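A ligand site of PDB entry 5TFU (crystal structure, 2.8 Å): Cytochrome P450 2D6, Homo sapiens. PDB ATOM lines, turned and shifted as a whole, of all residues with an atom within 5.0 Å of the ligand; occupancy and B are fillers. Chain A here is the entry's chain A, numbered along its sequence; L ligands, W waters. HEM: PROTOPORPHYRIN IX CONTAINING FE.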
ATOM      1  N   LEU A  69       8.222 -29.163  32.804  1.00  0.00           N
ATOM      2  CA  LEU A  69       8.390 -27.741  32.536  1.00  0.00           C
ATOM      3  C   LEU A  69       7.126 -27.066  32.002  1.00  0.00           C
ATOM      4  O   LEU A  69       6.992 -25.843  32.096  1.00  0.00           O
ATOM      5  CB  LEU A  69       9.535 -27.531  31.533  1.00  0.00           C
ATOM      6  CG  LEU A  69      10.898 -28.055  31.991  1.00  0.00           C
ATOM      7  CD1 LEU A  69      11.967 -27.661  30.984  1.00  0.00           C
ATOM      8  CD2 LEU A  69      11.245 -27.542  33.373  1.00  0.00           C
ATOM      9  N   ARG A  79      14.740 -22.112  40.921  1.00  0.00           N
ATOM     10  CA  ARG A  79      16.148 -22.467  40.850  1.00  0.00           C
ATOM     11  C   ARG A  79      16.644 -23.006  42.196  1.00  0.00           C
ATOM     12  O   ARG A  79      16.170 -22.579  43.243  1.00  0.00           O
ATOM     13  CB  ARG A  79      16.999 -21.260  40.438  1.00  0.00           C
ATOM     14  CG  ARG A  79      16.608 -20.622  39.123  1.00  0.00           C
ATOM     15  CD  ARG A  79      16.882 -21.529  37.950  1.00  0.00           C
ATOM     16  NE  ARG A  79      16.666 -20.850  36.678  1.00  0.00           N
ATOM     17  CZ  ARG A  79      16.674 -21.455  35.497  1.00  0.00           C
ATOM     18  NH1 ARG A  79      16.463 -20.758  34.387  1.00  0.00           N
ATOM     19  NH2 ARG A  79      16.892 -22.766  35.414  1.00  0.00           N
ATOM     20  N   VAL A  97      18.171 -12.498  36.794  1.00  0.00           N
ATOM     21  CA  VAL A  97      17.146 -13.268  36.102  1.00  0.00           C
ATOM     22  C   VAL A  97      17.496 -14.750  36.074  1.00  0.00           C
ATOM     23  O   VAL A  97      16.677 -15.604  36.392  1.00  0.00           O
ATOM     24  CB  VAL A  97      16.951 -12.782  34.656  1.00  0.00           C
ATOM     25  CG1 VAL A  97      15.879 -13.609  33.962  1.00  0.00           C
ATOM     26  CG2 VAL A  97      16.580 -11.304  34.639  1.00  0.00           C
ATOM     27  N   PHE A  98      18.742 -15.038  35.686  1.00  0.00           N
ATOM     28  CA  PHE A  98      19.189 -16.398  35.417  1.00  0.00           C
ATOM     29  C   PHE A  98      19.081 -17.320  36.627  1.00  0.00           C
ATOM     30  O   PHE A  98      18.531 -18.414  36.529  1.00  0.00           O
ATOM     31  CB  PHE A  98      20.619 -16.385  34.899  1.00  0.00           C
ATOM     32  CG  PHE A  98      21.093 -17.698  34.352  1.00  0.00           C
ATOM     33  CD1 PHE A  98      20.765 -18.078  33.055  1.00  0.00           C
ATOM     34  CD2 PHE A  98      21.848 -18.555  35.126  1.00  0.00           C
ATOM     35  CE1 PHE A  98      21.189 -19.288  32.550  1.00  0.00           C
ATOM     36  CE2 PHE A  98      22.277 -19.766  34.629  1.00  0.00           C
ATOM     37  CZ  PHE A  98      21.954 -20.132  33.331  1.00  0.00           C
ATOM     38  N   TRP A 106      11.975 -12.538  40.331  1.00  0.00           N
ATOM     39  CA  TRP A 106      12.266 -13.106  39.024  1.00  0.00           C
ATOM     40  C   TRP A 106      11.277 -12.650  37.967  1.00  0.00           C
ATOM     41  O   TRP A 106      11.668 -12.271  36.865  1.00  0.00           O
ATOM     42  CB  TRP A 106      12.261 -14.637  39.091  1.00  0.00           C
ATOM     43  CG  TRP A 106      12.258 -15.282  37.738  1.00  0.00           C
ATOM     44  CD1 TRP A 106      13.341 -15.545  36.947  1.00  0.00           C
ATOM     45  CD2 TRP A 106      11.110 -15.743  37.014  1.00  0.00           C
ATOM     46  NE1 TRP A 106      12.942 -16.134  35.773  1.00  0.00           N
ATOM     47  CE2 TRP A 106      11.578 -16.260  35.785  1.00  0.00           C
ATOM     48  CE3 TRP A 106       9.741 -15.759  37.275  1.00  0.00           C
ATOM     49  CZ2 TRP A 106      10.713 -16.806  34.829  1.00  0.00           C
ATOM     50  CZ3 TRP A 106       8.887 -16.293  36.326  1.00  0.00           C
ATOM     51  CH2 TRP A 106       9.377 -16.809  35.118  1.00  0.00           C
ATOM     52  N   ARG A 110      12.143 -10.848  34.591  1.00  0.00           N
ATOM     53  CA  ARG A 110      11.828 -11.664  33.422  1.00  0.00           C
ATOM     54  C   ARG A 110      10.942 -10.900  32.458  1.00  0.00           C
ATOM     55  O   ARG A 110      11.243 -10.781  31.261  1.00  0.00           O
ATOM     56  CB  ARG A 110      11.145 -12.962  33.842  1.00  0.00           C
ATOM     57  CG  ARG A 110      10.567 -13.775  32.688  1.00  0.00           C
ATOM     58  CD  ARG A 110      11.619 -14.668  32.051  1.00  0.00           C
ATOM     59  NE  ARG A 110      11.106 -15.343  30.863  1.00  0.00           N
ATOM     60  CZ  ARG A 110      11.693 -16.383  30.282  1.00  0.00           C
ATOM     61  NH1 ARG A 110      12.810 -16.885  30.782  1.00  0.00           N
ATOM     62  NH2 ARG A 110      11.159 -16.929  29.191  1.00  0.00           N
ATOM     63  N   LEU A 117      13.412  -6.302  25.125  1.00  0.00           N
ATOM     64  CA  LEU A 117      13.959  -6.896  23.911  1.00  0.00           C
ATOM     65  C   LEU A 117      12.977  -6.756  22.754  1.00  0.00           C
ATOM     66  O   LEU A 117      13.366  -6.479  21.629  1.00  0.00           O
ATOM     67  CB  LEU A 117      14.295  -8.380  24.133  1.00  0.00           C
ATOM     68  CG  LEU A 117      15.548  -8.723  24.933  1.00  0.00           C
ATOM     69  CD1 LEU A 117      15.647 -10.224  25.153  1.00  0.00           C
ATOM     70  CD2 LEU A 117      16.797  -8.194  24.245  1.00  0.00           C
ATOM     71  N   ILE A 164      25.031  -7.831  22.304  1.00  0.00           N
ATOM     72  CA  ILE A 164      24.501  -7.705  23.651  1.00  0.00           C
ATOM     73  C   ILE A 164      24.746  -6.310  24.219  1.00  0.00           C
ATOM     74  O   ILE A 164      23.842  -5.688  24.784  1.00  0.00           O
ATOM     75  CB  ILE A 164      25.129  -8.741  24.606  1.00  0.00           C
ATOM     76  CG1 ILE A 164      24.806 -10.153  24.128  1.00  0.00           C
ATOM     77  CG2 ILE A 164      24.605  -8.542  26.005  1.00  0.00           C
ATOM     78  CD1 ILE A 164      23.329 -10.478  24.148  1.00  0.00           C
ATOM     79  N   LEU A 280      22.399 -11.085  31.285  1.00  0.00           N
ATOM     80  CA  LEU A 280      22.116 -10.968  29.858  1.00  0.00           C
ATOM     81  C   LEU A 280      23.395 -10.999  29.039  1.00  0.00           C
ATOM     82  O   LEU A 280      23.444 -11.615  27.972  1.00  0.00           O
ATOM     83  CB  LEU A 280      21.354  -9.670  29.570  1.00  0.00           C
ATOM     84  CG  LEU A 280      20.005  -9.516  30.270  1.00  0.00           C
ATOM     85  CD1 LEU A 280      19.474  -8.116  30.093  1.00  0.00           C
ATOM     86  CD2 LEU A 280      19.020 -10.552  29.745  1.00  0.00           C
ATOM     87  N   ALA A 283      25.185 -14.669  29.298  1.00  0.00           N
ATOM     88  CA  ALA A 283      24.357 -15.716  28.715  1.00  0.00           C
ATOM     89  C   ALA A 283      24.401 -15.722  27.200  1.00  0.00           C
ATOM     90  O   ALA A 283      24.682 -16.756  26.577  1.00  0.00           O
ATOM     91  CB  ALA A 283      22.920 -15.568  29.198  1.00  0.00           C
ATOM     92  N   GLY A 284      24.123 -14.573  26.589  1.00  0.00           N
ATOM     93  CA  GLY A 284      24.084 -14.475  25.146  1.00  0.00           C
ATOM     94  C   GLY A 284      25.413 -14.085  24.534  1.00  0.00           C
ATOM     95  O   GLY A 284      25.475 -13.271  23.604  1.00  0.00           O
ATOM     96  N   THR A 287      26.961 -18.665  24.536  1.00  0.00           N
ATOM     97  CA  THR A 287      26.061 -19.600  23.868  1.00  0.00           C
ATOM     98  C   THR A 287      26.016 -19.344  22.366  1.00  0.00           C
ATOM     99  O   THR A 287      26.352 -20.223  21.566  1.00  0.00           O
ATOM    100  CB  THR A 287      24.629 -19.497  24.436  1.00  0.00           C
ATOM    101  OG1 THR A 287      24.177 -18.142  24.346  1.00  0.00           O
ATOM    102  CG2 THR A 287      24.601 -19.945  25.888  1.00  0.00           C
ATOM    103  N   THR A 288      25.614 -18.138  21.986  1.00  0.00           N
ATOM    104  CA  THR A 288      25.460 -17.771  20.582  1.00  0.00           C
ATOM    105  C   THR A 288      26.775 -17.873  19.816  1.00  0.00           C
ATOM    106  O   THR A 288      26.799 -18.222  18.633  1.00  0.00           O
ATOM    107  CB  THR A 288      24.907 -16.342  20.433  1.00  0.00           C
ATOM    108  OG1 THR A 288      23.860 -16.137  21.381  1.00  0.00           O
ATOM    109  CG2 THR A 288      24.377 -16.120  19.023  1.00  0.00           C
ATOM    110  N   THR A 291      27.654 -21.631  19.362  1.00  0.00           N
ATOM    111  CA  THR A 291      26.793 -22.145  18.303  1.00  0.00           C
ATOM    112  C   THR A 291      27.368 -21.806  16.937  1.00  0.00           C
ATOM    113  O   THR A 291      27.482 -22.678  16.070  1.00  0.00           O
ATOM    114  CB  THR A 291      25.368 -21.579  18.409  1.00  0.00           C
ATOM    115  OG1 THR A 291      24.797 -21.949  19.664  1.00  0.00           O
ATOM    116  CG2 THR A 291      24.504 -22.130  17.289  1.00  0.00           C
ATOM    117  N   GLN A 342      22.283 -26.097  15.778  1.00  0.00           N
ATOM    118  CA  GLN A 342      21.876 -26.070  17.182  1.00  0.00           C
ATOM    119  C   GLN A 342      21.607 -27.480  17.708  1.00  0.00           C
ATOM    120  O   GLN A 342      22.032 -27.836  18.803  1.00  0.00           O
ATOM    121  CB  GLN A 342      20.636 -25.191  17.380  1.00  0.00           C
ATOM    122  CG  GLN A 342      20.880 -23.708  17.168  1.00  0.00           C
ATOM    123  CD  GLN A 342      19.799 -22.842  17.795  1.00  0.00           C
ATOM    124  OE1 GLN A 342      18.851 -22.424  17.128  1.00  0.00           O
ATOM    125  NE2 GLN A 342      19.937 -22.562  19.085  1.00  0.00           N
ATOM    126  N   ILE A 347      24.805 -27.522  22.587  1.00  0.00           N
ATOM    127  CA  ILE A 347      25.787 -26.812  23.401  1.00  0.00           C
ATOM    128  C   ILE A 347      25.431 -26.826  24.887  1.00  0.00           C
ATOM    129  O   ILE A 347      26.320 -26.742  25.740  1.00  0.00           O
ATOM    130  CB  ILE A 347      25.953 -25.351  22.930  1.00  0.00           C
ATOM    131  CG1 ILE A 347      24.674 -24.546  23.153  1.00  0.00           C
ATOM    132  CG2 ILE A 347      26.332 -25.322  21.455  1.00  0.00           C
ATOM    133  CD1 ILE A 347      24.846 -23.058  22.925  1.00  0.00           C
ATOM    134  N   VAL A 348      24.148 -26.940  25.202  1.00  0.00           N
ATOM    135  CA  VAL A 348      23.708 -27.062  26.596  1.00  0.00           C
ATOM    136  C   VAL A 348      23.019 -28.402  26.782  1.00  0.00           C
ATOM    137  O   VAL A 348      21.795 -28.483  26.753  1.00  0.00           O
ATOM    138  CB  VAL A 348      22.753 -25.920  27.008  1.00  0.00           C
ATOM    139  CG1 VAL A 348      22.768 -25.754  28.520  1.00  0.00           C
ATOM    140  CG2 VAL A 348      23.146 -24.626  26.338  1.00  0.00           C
ATOM    141  N   GLY A 351      21.064 -28.674  30.147  1.00  0.00           N
ATOM    142  CA  GLY A 351      20.287 -27.474  30.392  1.00  0.00           C
ATOM    143  C   GLY A 351      20.750 -26.713  31.607  1.00  0.00           C
ATOM    144  O   GLY A 351      21.923 -26.797  31.996  1.00  0.00           O
ATOM    145  N   VAL A 352      19.839 -25.975  32.213  1.00  0.00           N
ATOM    146  CA  VAL A 352      20.122 -25.281  33.468  1.00  0.00           C
ATOM    147  C   VAL A 352      19.201 -25.867  34.541  1.00  0.00           C
ATOM    148  O   VAL A 352      18.004 -25.992  34.316  1.00  0.00           O
ATOM    149  CB  VAL A 352      19.908 -23.767  33.340  1.00  0.00           C
ATOM    150  CG1 VAL A 352      20.182 -23.076  34.669  1.00  0.00           C
ATOM    151  CG2 VAL A 352      20.813 -23.206  32.262  1.00  0.00           C
ATOM    152  N   HIS A 354      16.719 -26.962  37.348  1.00  0.00           N
ATOM    153  CA  HIS A 354      15.491 -26.442  37.927  1.00  0.00           C
ATOM    154  C   HIS A 354      15.329 -26.984  39.342  1.00  0.00           C
ATOM    155  O   HIS A 354      16.176 -27.747  39.817  1.00  0.00           O
ATOM    156  CB  HIS A 354      14.271 -26.835  37.079  1.00  0.00           C
ATOM    157  CG  HIS A 354      14.215 -26.127  35.764  1.00  0.00           C
ATOM    158  ND1 HIS A 354      13.184 -25.278  35.430  1.00  0.00           N
ATOM    159  CD2 HIS A 354      15.041 -26.148  34.698  1.00  0.00           C
ATOM    160  CE1 HIS A 354      13.383 -24.795  34.218  1.00  0.00           C
ATOM    161  NE2 HIS A 354      14.508 -25.313  33.746  1.00  0.00           N
ATOM    162  N   LEU A 377      18.476 -32.014  27.935  1.00  0.00           N
ATOM    163  CA  LEU A 377      18.091 -31.516  26.624  1.00  0.00           C
ATOM    164  C   LEU A 377      18.742 -32.325  25.510  1.00  0.00           C
ATOM    165  O   LEU A 377      18.200 -32.460  24.414  1.00  0.00           O
ATOM    166  CB  LEU A 377      18.445 -30.040  26.475  1.00  0.00           C
ATOM    167  CG  LEU A 377      17.785 -29.079  27.473  1.00  0.00           C
ATOM    168  CD1 LEU A 377      18.267 -27.659  27.242  1.00  0.00           C
ATOM    169  CD2 LEU A 377      16.267 -29.146  27.384  1.00  0.00           C
ATOM    170  N   PRO A 413      16.475 -26.600  22.094  1.00  0.00           N
ATOM    171  CA  PRO A 413      17.792 -26.163  22.564  1.00  0.00           C
ATOM    172  C   PRO A 413      17.680 -25.034  23.589  1.00  0.00           C
ATOM    173  O   PRO A 413      18.617 -24.802  24.361  1.00  0.00           O
ATOM    174  CB  PRO A 413      18.468 -25.678  21.285  1.00  0.00           C
ATOM    175  CG  PRO A 413      17.342 -25.185  20.440  1.00  0.00           C
ATOM    176  CD  PRO A 413      16.180 -26.106  20.742  1.00  0.00           C
ATOM    177  N   PHE A 414      16.538 -24.342  23.602  1.00  0.00           N
ATOM    178  CA  PHE A 414      16.300 -23.262  24.555  1.00  0.00           C
ATOM    179  C   PHE A 414      15.421 -23.740  25.709  1.00  0.00           C
ATOM    180  O   PHE A 414      14.819 -22.925  26.412  1.00  0.00           O
ATOM    181  CB  PHE A 414      15.624 -22.081  23.866  1.00  0.00           C
ATOM    182  CG  PHE A 414      16.415 -21.512  22.716  1.00  0.00           C
ATOM    183  CD1 PHE A 414      16.018 -21.756  21.406  1.00  0.00           C
ATOM    184  CD2 PHE A 414      17.536 -20.738  22.944  1.00  0.00           C
ATOM    185  CE1 PHE A 414      16.736 -21.238  20.350  1.00  0.00           C
ATOM    186  CE2 PHE A 414      18.261 -20.216  21.885  1.00  0.00           C
ATOM    187  CZ  PHE A 414      17.856 -20.464  20.579  1.00  0.00           C
ATOM    188  N   SER A 415      15.365 -25.058  25.889  1.00  0.00           N
ATOM    189  CA  SER A 415      14.504 -25.688  26.875  1.00  0.00           C
ATOM    190  C   SER A 415      13.043 -25.317  26.653  1.00  0.00           C
ATOM    191  O   SER A 415      12.645 -24.959  25.543  1.00  0.00           O
ATOM    192  CB  SER A 415      14.936 -25.313  28.296  1.00  0.00           C
ATOM    193  OG  SER A 415      14.177 -26.003  29.263  1.00  0.00           O
ATOM    194  N   ALA A 416      12.239 -25.416  27.704  1.00  0.00           N
ATOM    195  CA  ALA A 416      10.809 -25.095  27.609  1.00  0.00           C
ATOM    196  C   ALA A 416      10.255 -24.615  28.943  1.00  0.00           C
ATOM    197  O   ALA A 416      10.925 -24.703  29.973  1.00  0.00           O
ATOM    198  CB  ALA A 416      10.031 -26.306  27.118  1.00  0.00           C
ATOM    199  N   ARG A 418       8.263 -21.800  31.668  1.00  0.00           N
ATOM    200  CA  ARG A 418       8.410 -20.410  32.117  1.00  0.00           C
ATOM    201  C   ARG A 418       9.872 -19.959  32.133  1.00  0.00           C
ATOM    202  O   ARG A 418      10.153 -18.783  31.933  1.00  0.00           O
ATOM    203  CB  ARG A 418       7.803 -20.247  33.514  1.00  0.00           C
ATOM    204  CG  ARG A 418       6.283 -20.337  33.540  1.00  0.00           C
ATOM    205  CD  ARG A 418       5.753 -20.364  34.963  1.00  0.00           C
ATOM    206  NE  ARG A 418       4.320 -20.109  35.014  1.00  0.00           N
ATOM    207  CZ  ARG A 418       3.391 -21.050  34.887  1.00  0.00           C
ATOM    208  NH1 ARG A 418       2.107 -20.718  34.941  1.00  0.00           N
ATOM    209  NH2 ARG A 418       3.743 -22.312  34.707  1.00  0.00           N
ATOM    210  N   ARG A 419      10.774 -20.892  32.358  1.00  0.00           N
ATOM    211  CA  ARG A 419      12.198 -20.576  32.462  1.00  0.00           C
ATOM    212  C   ARG A 419      12.935 -20.677  31.136  1.00  0.00           C
ATOM    213  O   ARG A 419      14.154 -20.501  31.098  1.00  0.00           O
ATOM    214  CB  ARG A 419      12.860 -21.493  33.492  1.00  0.00           C
ATOM    215  CG  ARG A 419      12.588 -21.109  34.929  1.00  0.00           C
ATOM    216  CD  ARG A 419      13.367 -19.861  35.296  1.00  0.00           C
ATOM    217  NE  ARG A 419      13.246 -19.557  36.717  1.00  0.00           N
ATOM    218  CZ  ARG A 419      14.079 -18.772  37.383  1.00  0.00           C
ATOM    219  NH1 ARG A 419      15.109 -18.198  36.757  1.00  0.00           N
ATOM    220  NH2 ARG A 419      13.893 -18.549  38.681  1.00  0.00           N
ATOM    221  N   ALA A 420      12.203 -20.953  30.064  1.00  0.00           N
ATOM    222  CA  ALA A 420      12.799 -21.065  28.738  1.00  0.00           C
ATOM    223  C   ALA A 420      13.570 -19.794  28.392  1.00  0.00           C
ATOM    224  O   ALA A 420      13.197 -18.708  28.818  1.00  0.00           O
ATOM    225  CB  ALA A 420      11.726 -21.343  27.690  1.00  0.00           C
ATOM    226  N   CYS A 421      14.646 -19.958  27.629  1.00  0.00           N
ATOM    227  CA  CYS A 421      15.542 -18.867  27.247  1.00  0.00           C
ATOM    228  C   CYS A 421      14.795 -17.650  26.732  1.00  0.00           C
ATOM    229  O   CYS A 421      14.044 -17.744  25.762  1.00  0.00           O
ATOM    230  CB  CYS A 421      16.532 -19.363  26.193  1.00  0.00           C
ATOM    231  SG  CYS A 421      17.798 -18.169  25.700  1.00  0.00           S
ATOM    232  N   LEU A 422      14.985 -16.506  27.395  1.00  0.00           N
ATOM    233  CA  LEU A 422      14.317 -15.271  26.975  1.00  0.00           C
ATOM    234  C   LEU A 422      15.086 -14.615  25.837  1.00  0.00           C
ATOM    235  O   LEU A 422      14.616 -13.647  25.236  1.00  0.00           O
ATOM    236  CB  LEU A 422      14.172 -14.308  28.162  1.00  0.00           C
ATOM    237  CG  LEU A 422      15.397 -13.795  28.939  1.00  0.00           C
ATOM    238  CD1 LEU A 422      16.091 -12.629  28.242  1.00  0.00           C
ATOM    239  CD2 LEU A 422      14.995 -13.399  30.349  1.00  0.00           C
ATOM    240  N   GLY A 423      16.273 -15.135  25.549  1.00  0.00           N
ATOM    241  CA  GLY A 423      17.112 -14.587  24.519  1.00  0.00           C
ATOM    242  C   GLY A 423      16.932 -15.265  23.172  1.00  0.00           C
ATOM    243  O   GLY A 423      17.599 -14.916  22.196  1.00  0.00           O
ATOM    244  N   LEU A 426      16.386 -13.108  20.044  1.00  0.00           N
ATOM    245  CA  LEU A 426      17.643 -12.452  19.668  1.00  0.00           C
ATOM    246  C   LEU A 426      18.623 -13.447  19.084  1.00  0.00           C
ATOM    247  O   LEU A 426      19.293 -13.170  18.098  1.00  0.00           O
ATOM    248  CB  LEU A 426      18.265 -11.750  20.877  1.00  0.00           C
ATOM    249  CG  LEU A 426      19.614 -11.087  20.610  1.00  0.00           C
ATOM    250  CD1 LEU A 426      19.451  -9.903  19.670  1.00  0.00           C
ATOM    251  CD2 LEU A 426      20.278 -10.661  21.914  1.00  0.00           C
ATOM    252  N   ALA A 427      18.687 -14.630  19.699  1.00  0.00           N
ATOM    253  CA  ALA A 427      19.548 -15.708  19.234  1.00  0.00           C
ATOM    254  C   ALA A 427      19.202 -16.106  17.794  1.00  0.00           C
ATOM    255  O   ALA A 427      20.089 -16.217  16.950  1.00  0.00           O
ATOM    256  CB  ALA A 427      19.441 -16.914  20.154  1.00  0.00           C
ATOM    257  N   GLU A 430      20.509 -13.316  15.650  1.00  0.00           N
ATOM    258  CA  GLU A 430      21.966 -13.343  15.589  1.00  0.00           C
ATOM    259  C   GLU A 430      22.481 -14.502  14.745  1.00  0.00           C
ATOM    260  O   GLU A 430      23.393 -14.325  13.944  1.00  0.00           O
ATOM    261  CB  GLU A 430      22.569 -13.434  16.996  1.00  0.00           C
ATOM    262  CG  GLU A 430      22.480 -12.156  17.802  1.00  0.00           C
ATOM    263  CD  GLU A 430      23.340 -12.219  19.050  1.00  0.00           C
ATOM    264  OE1 GLU A 430      24.564 -12.000  18.945  1.00  0.00           O
ATOM    265  OE2 GLU A 430      22.797 -12.498  20.137  1.00  0.00           O
ATOM    266  N   LEU A 431      21.880 -15.671  14.923  1.00  0.00           N
ATOM    267  CA  LEU A 431      22.318 -16.867  14.202  1.00  0.00           C
ATOM    268  C   LEU A 431      22.099 -16.731  12.705  1.00  0.00           C
ATOM    269  O   LEU A 431      23.016 -16.971  11.921  1.00  0.00           O
ATOM    270  CB  LEU A 431      21.591 -18.111  14.724  1.00  0.00           C
ATOM    271  CG  LEU A 431      22.037 -18.579  16.107  1.00  0.00           C
ATOM    272  CD1 LEU A 431      21.277 -19.837  16.531  1.00  0.00           C
ATOM    273  CD2 LEU A 431      23.532 -18.818  16.139  1.00  0.00           C
HETATM  274  CHA HEM L   1      18.104 -19.501  29.832  1.00  0.00           C
HETATM  275  CHB HEM L   1      19.942 -21.716  25.906  1.00  0.00           C
HETATM  276  CHC HEM L   1      21.103 -17.373  24.053  1.00  0.00           C
HETATM  277  CHD HEM L   1      19.681 -15.230  28.170  1.00  0.00           C
HETATM  278  C1A HEM L   1      18.527 -20.480  28.947  1.00  0.00           C
HETATM  279  C2A HEM L   1      18.425 -21.908  29.153  1.00  0.00           C
HETATM  280  C3A HEM L   1      18.929 -22.526  28.088  1.00  0.00           C
HETATM  281  C4A HEM L   1      19.363 -21.507  27.141  1.00  0.00           C
HETATM  282  CMA HEM L   1      19.018 -24.014  27.885  1.00  0.00           C
HETATM  283  CAA HEM L   1      17.839 -22.578  30.416  1.00  0.00           C
HETATM  284  CBA HEM L   1      16.317 -22.665  30.281  1.00  0.00           C
HETATM  285  CGA HEM L   1      15.728 -23.267  31.530  1.00  0.00           C
HETATM  286  O1A HEM L   1      16.256 -22.978  32.641  1.00  0.00           O
HETATM  287  O2A HEM L   1      14.734 -24.024  31.416  1.00  0.00           O
HETATM  288  C1B HEM L   1      20.407 -20.736  25.052  1.00  0.00           C
HETATM  289  C2B HEM L   1      20.998 -20.951  23.740  1.00  0.00           C
HETATM  290  C3B HEM L   1      21.323 -19.756  23.226  1.00  0.00           C
HETATM  291  C4B HEM L   1      20.940 -18.736  24.197  1.00  0.00           C
HETATM  292  CMB HEM L   1      21.185 -22.322  23.133  1.00  0.00           C
HETATM  293  CAB HEM L   1      21.968 -19.384  21.858  1.00  0.00           C
HETATM  294  CBB HEM L   1      22.273 -20.255  20.892  1.00  0.00           C
HETATM  295  C1C HEM L   1      20.744 -16.402  24.958  1.00  0.00           C
HETATM  296  C2C HEM L   1      20.673 -14.976  24.725  1.00  0.00           C
HETATM  297  C3C HEM L   1      20.284 -14.379  25.871  1.00  0.00           C
HETATM  298  C4C HEM L   1      20.091 -15.424  26.861  1.00  0.00           C
HETATM  299  CMC HEM L   1      21.005 -14.331  23.397  1.00  0.00           C
HETATM  300  CAC HEM L   1      20.037 -12.879  26.203  1.00  0.00           C
HETATM  301  CBC HEM L   1      20.142 -11.866  25.342  1.00  0.00           C
HETATM  302  C1D HEM L   1      19.121 -16.192  28.977  1.00  0.00           C
HETATM  303  C2D HEM L   1      18.526 -15.975  30.280  1.00  0.00           C
HETATM  304  C3D HEM L   1      18.093 -17.156  30.743  1.00  0.00           C
HETATM  305  C4D HEM L   1      18.391 -18.160  29.741  1.00  0.00           C
HETATM  306  CMD HEM L   1      18.411 -14.659  31.002  1.00  0.00           C
HETATM  307  CAD HEM L   1      17.384 -17.411  32.091  1.00  0.00           C
HETATM  308  CBD HEM L   1      15.895 -17.161  31.918  1.00  0.00           C
HETATM  309  CGD HEM L   1      15.171 -17.519  33.194  1.00  0.00           C
HETATM  310  O1D HEM L   1      13.931 -17.345  33.239  1.00  0.00           O
HETATM  311  O2D HEM L   1      15.841 -17.987  34.145  1.00  0.00           O
HETATM  312  NA  HEM L   1      19.094 -20.269  27.710  1.00  0.00           N
HETATM  313  NB  HEM L   1      20.395 -19.376  25.289  1.00  0.00           N
HETATM  314  NC  HEM L   1      20.377 -16.641  26.272  1.00  0.00           N
HETATM  315  ND  HEM L   1      19.021 -17.536  28.680  1.00  0.00           N
HETATM  316 FE   HEM L   1      19.687 -18.466  26.960  1.00  0.00          FE
HETATM  317  O   HOH W   1      22.486 -23.565  19.960  1.00  0.00           O
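O1D of the ligand lies within salt-bridge range of NH1 of Arg 110 (2.7 Å). NH1 of Arg 419 is in salt-bridge range of O2D of the ligand (2.7 Å). FE of the ligand is bound by SG of Cys 421 (2.3 Å). NE2 of His 354 sits at hydrogen-bond distance from O2A of the ligand, 2.7 Å away. An oxygen (O2A) of the ligand sits at hydrogen-bond distance from the side-chain hydroxyl (OG) of Ser 415 (3.0 Å). The guanidinium group (NH1) of Arg 79 lies within salt-bridge range of an oxygen (O1A) of the ligand. NE1 of Trp 106 sits at hydrogen-bond distance from O1D of the ligand, 3.0 Å away.
The side-chain hydroxyl of Thr 291 sits at hydrogen-bond distance from the backbone carbonyl oxygen of Thr 287 (3.0 Å). NE of Arg 79 lies within hydrogen-bond range of O of Phe 98 (3.1 Å). The side-chain hydroxyl of Thr 287 sits at hydrogen-bond distance from the backbone carbonyl oxygen of Ala 283 (2.7 Å). The guanidinium group (NH1) of Arg 419 lies within hydrogen-bond range of the backbone carbonyl oxygen (O) of Val 97 (3.1 Å). The side-chain sulfur (SG) of Cys 421 lies close to the backbone NH (N) of Gly 423 (3.4 Å). NH2 of Arg 110 lies close to O of Arg 418, at 3.5 Å. The backbone carbonyl oxygen (O) of Phe 414 sits at hydrogen-bond distance from the backbone NH (N) of Cys 421 (3.2 Å). NH1 of Arg 419 sits at hydrogen-bond distance from O of Phe 98, at 3.4 Å.
The backbone carbonyl oxygen of Val 97 lies close to an oxygen (O2D) of the ligand (3.4 Å). CD1 of Phe 98 touches CAD of the ligand (3.6 Å). CD1 of Ile 164 touches CBC of the ligand (3.7 Å). Ala 283 touches the ligand. CA of Gly 284 touches C2C of the ligand, 3.5 Å away. OG1 of Thr 287 touches CHC of the ligand, 3.2 Å away. Thr 288 touches the ligand. Thr 291 touches the ligand (OG1 to CBB, 3.3 Å). Gln 342 touches the ligand (NE2 to CBB, 3.7 Å). Ile 347 touches the ligand (CD1 to CMB, 3.7 Å). Val 352 touches the ligand (CG2 to CAA, 3.6 Å). Leu 377 touches the ligand. O of Pro 413 touches CMA of the ligand, at 3.6 Å. Phe 414 touches the ligand (CE2 to C3B, 3.4 Å). Leu 422 touches the ligand. Gly 423 touches the ligand (CA to C3C, 3.5 Å). CD2 of Leu 426 touches CBC of the ligand, at 3.6 Å. CB of Ala 427 touches CAB of the ligand, at 3.9 Å. Hydrophobic or aromatic side chains within 4 Å of the ligand: Phe 98, Trp 106, Ile 164, Ala 283, Ile 347, Val 352, His 354, Leu 377, Phe 414, Leu 422, Leu 426 and Ala 427. 25 residues have an atom within 4 Å of the ligand: Arg 79, Val 97, Phe 98, Trp 106, Arg 110, Ile 164, Ala 283, Gly 284, Thr 287, Thr 288, Thr 291, Gln 342, Ile 347, Val 352, His 354, Leu 377, Pro 413, Phe 414, Ser 415, Arg 419, Cys 421, Leu 422, Gly 423, Leu 426 and Ala 427.
Water W1 lies within hydrogen-bond range of the side-chain hydroxyl (OG1) of Thr 291 (2.8 Å) and the side-chain amide nitrogen (NE2) of Gln 342 (2.9 Å).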
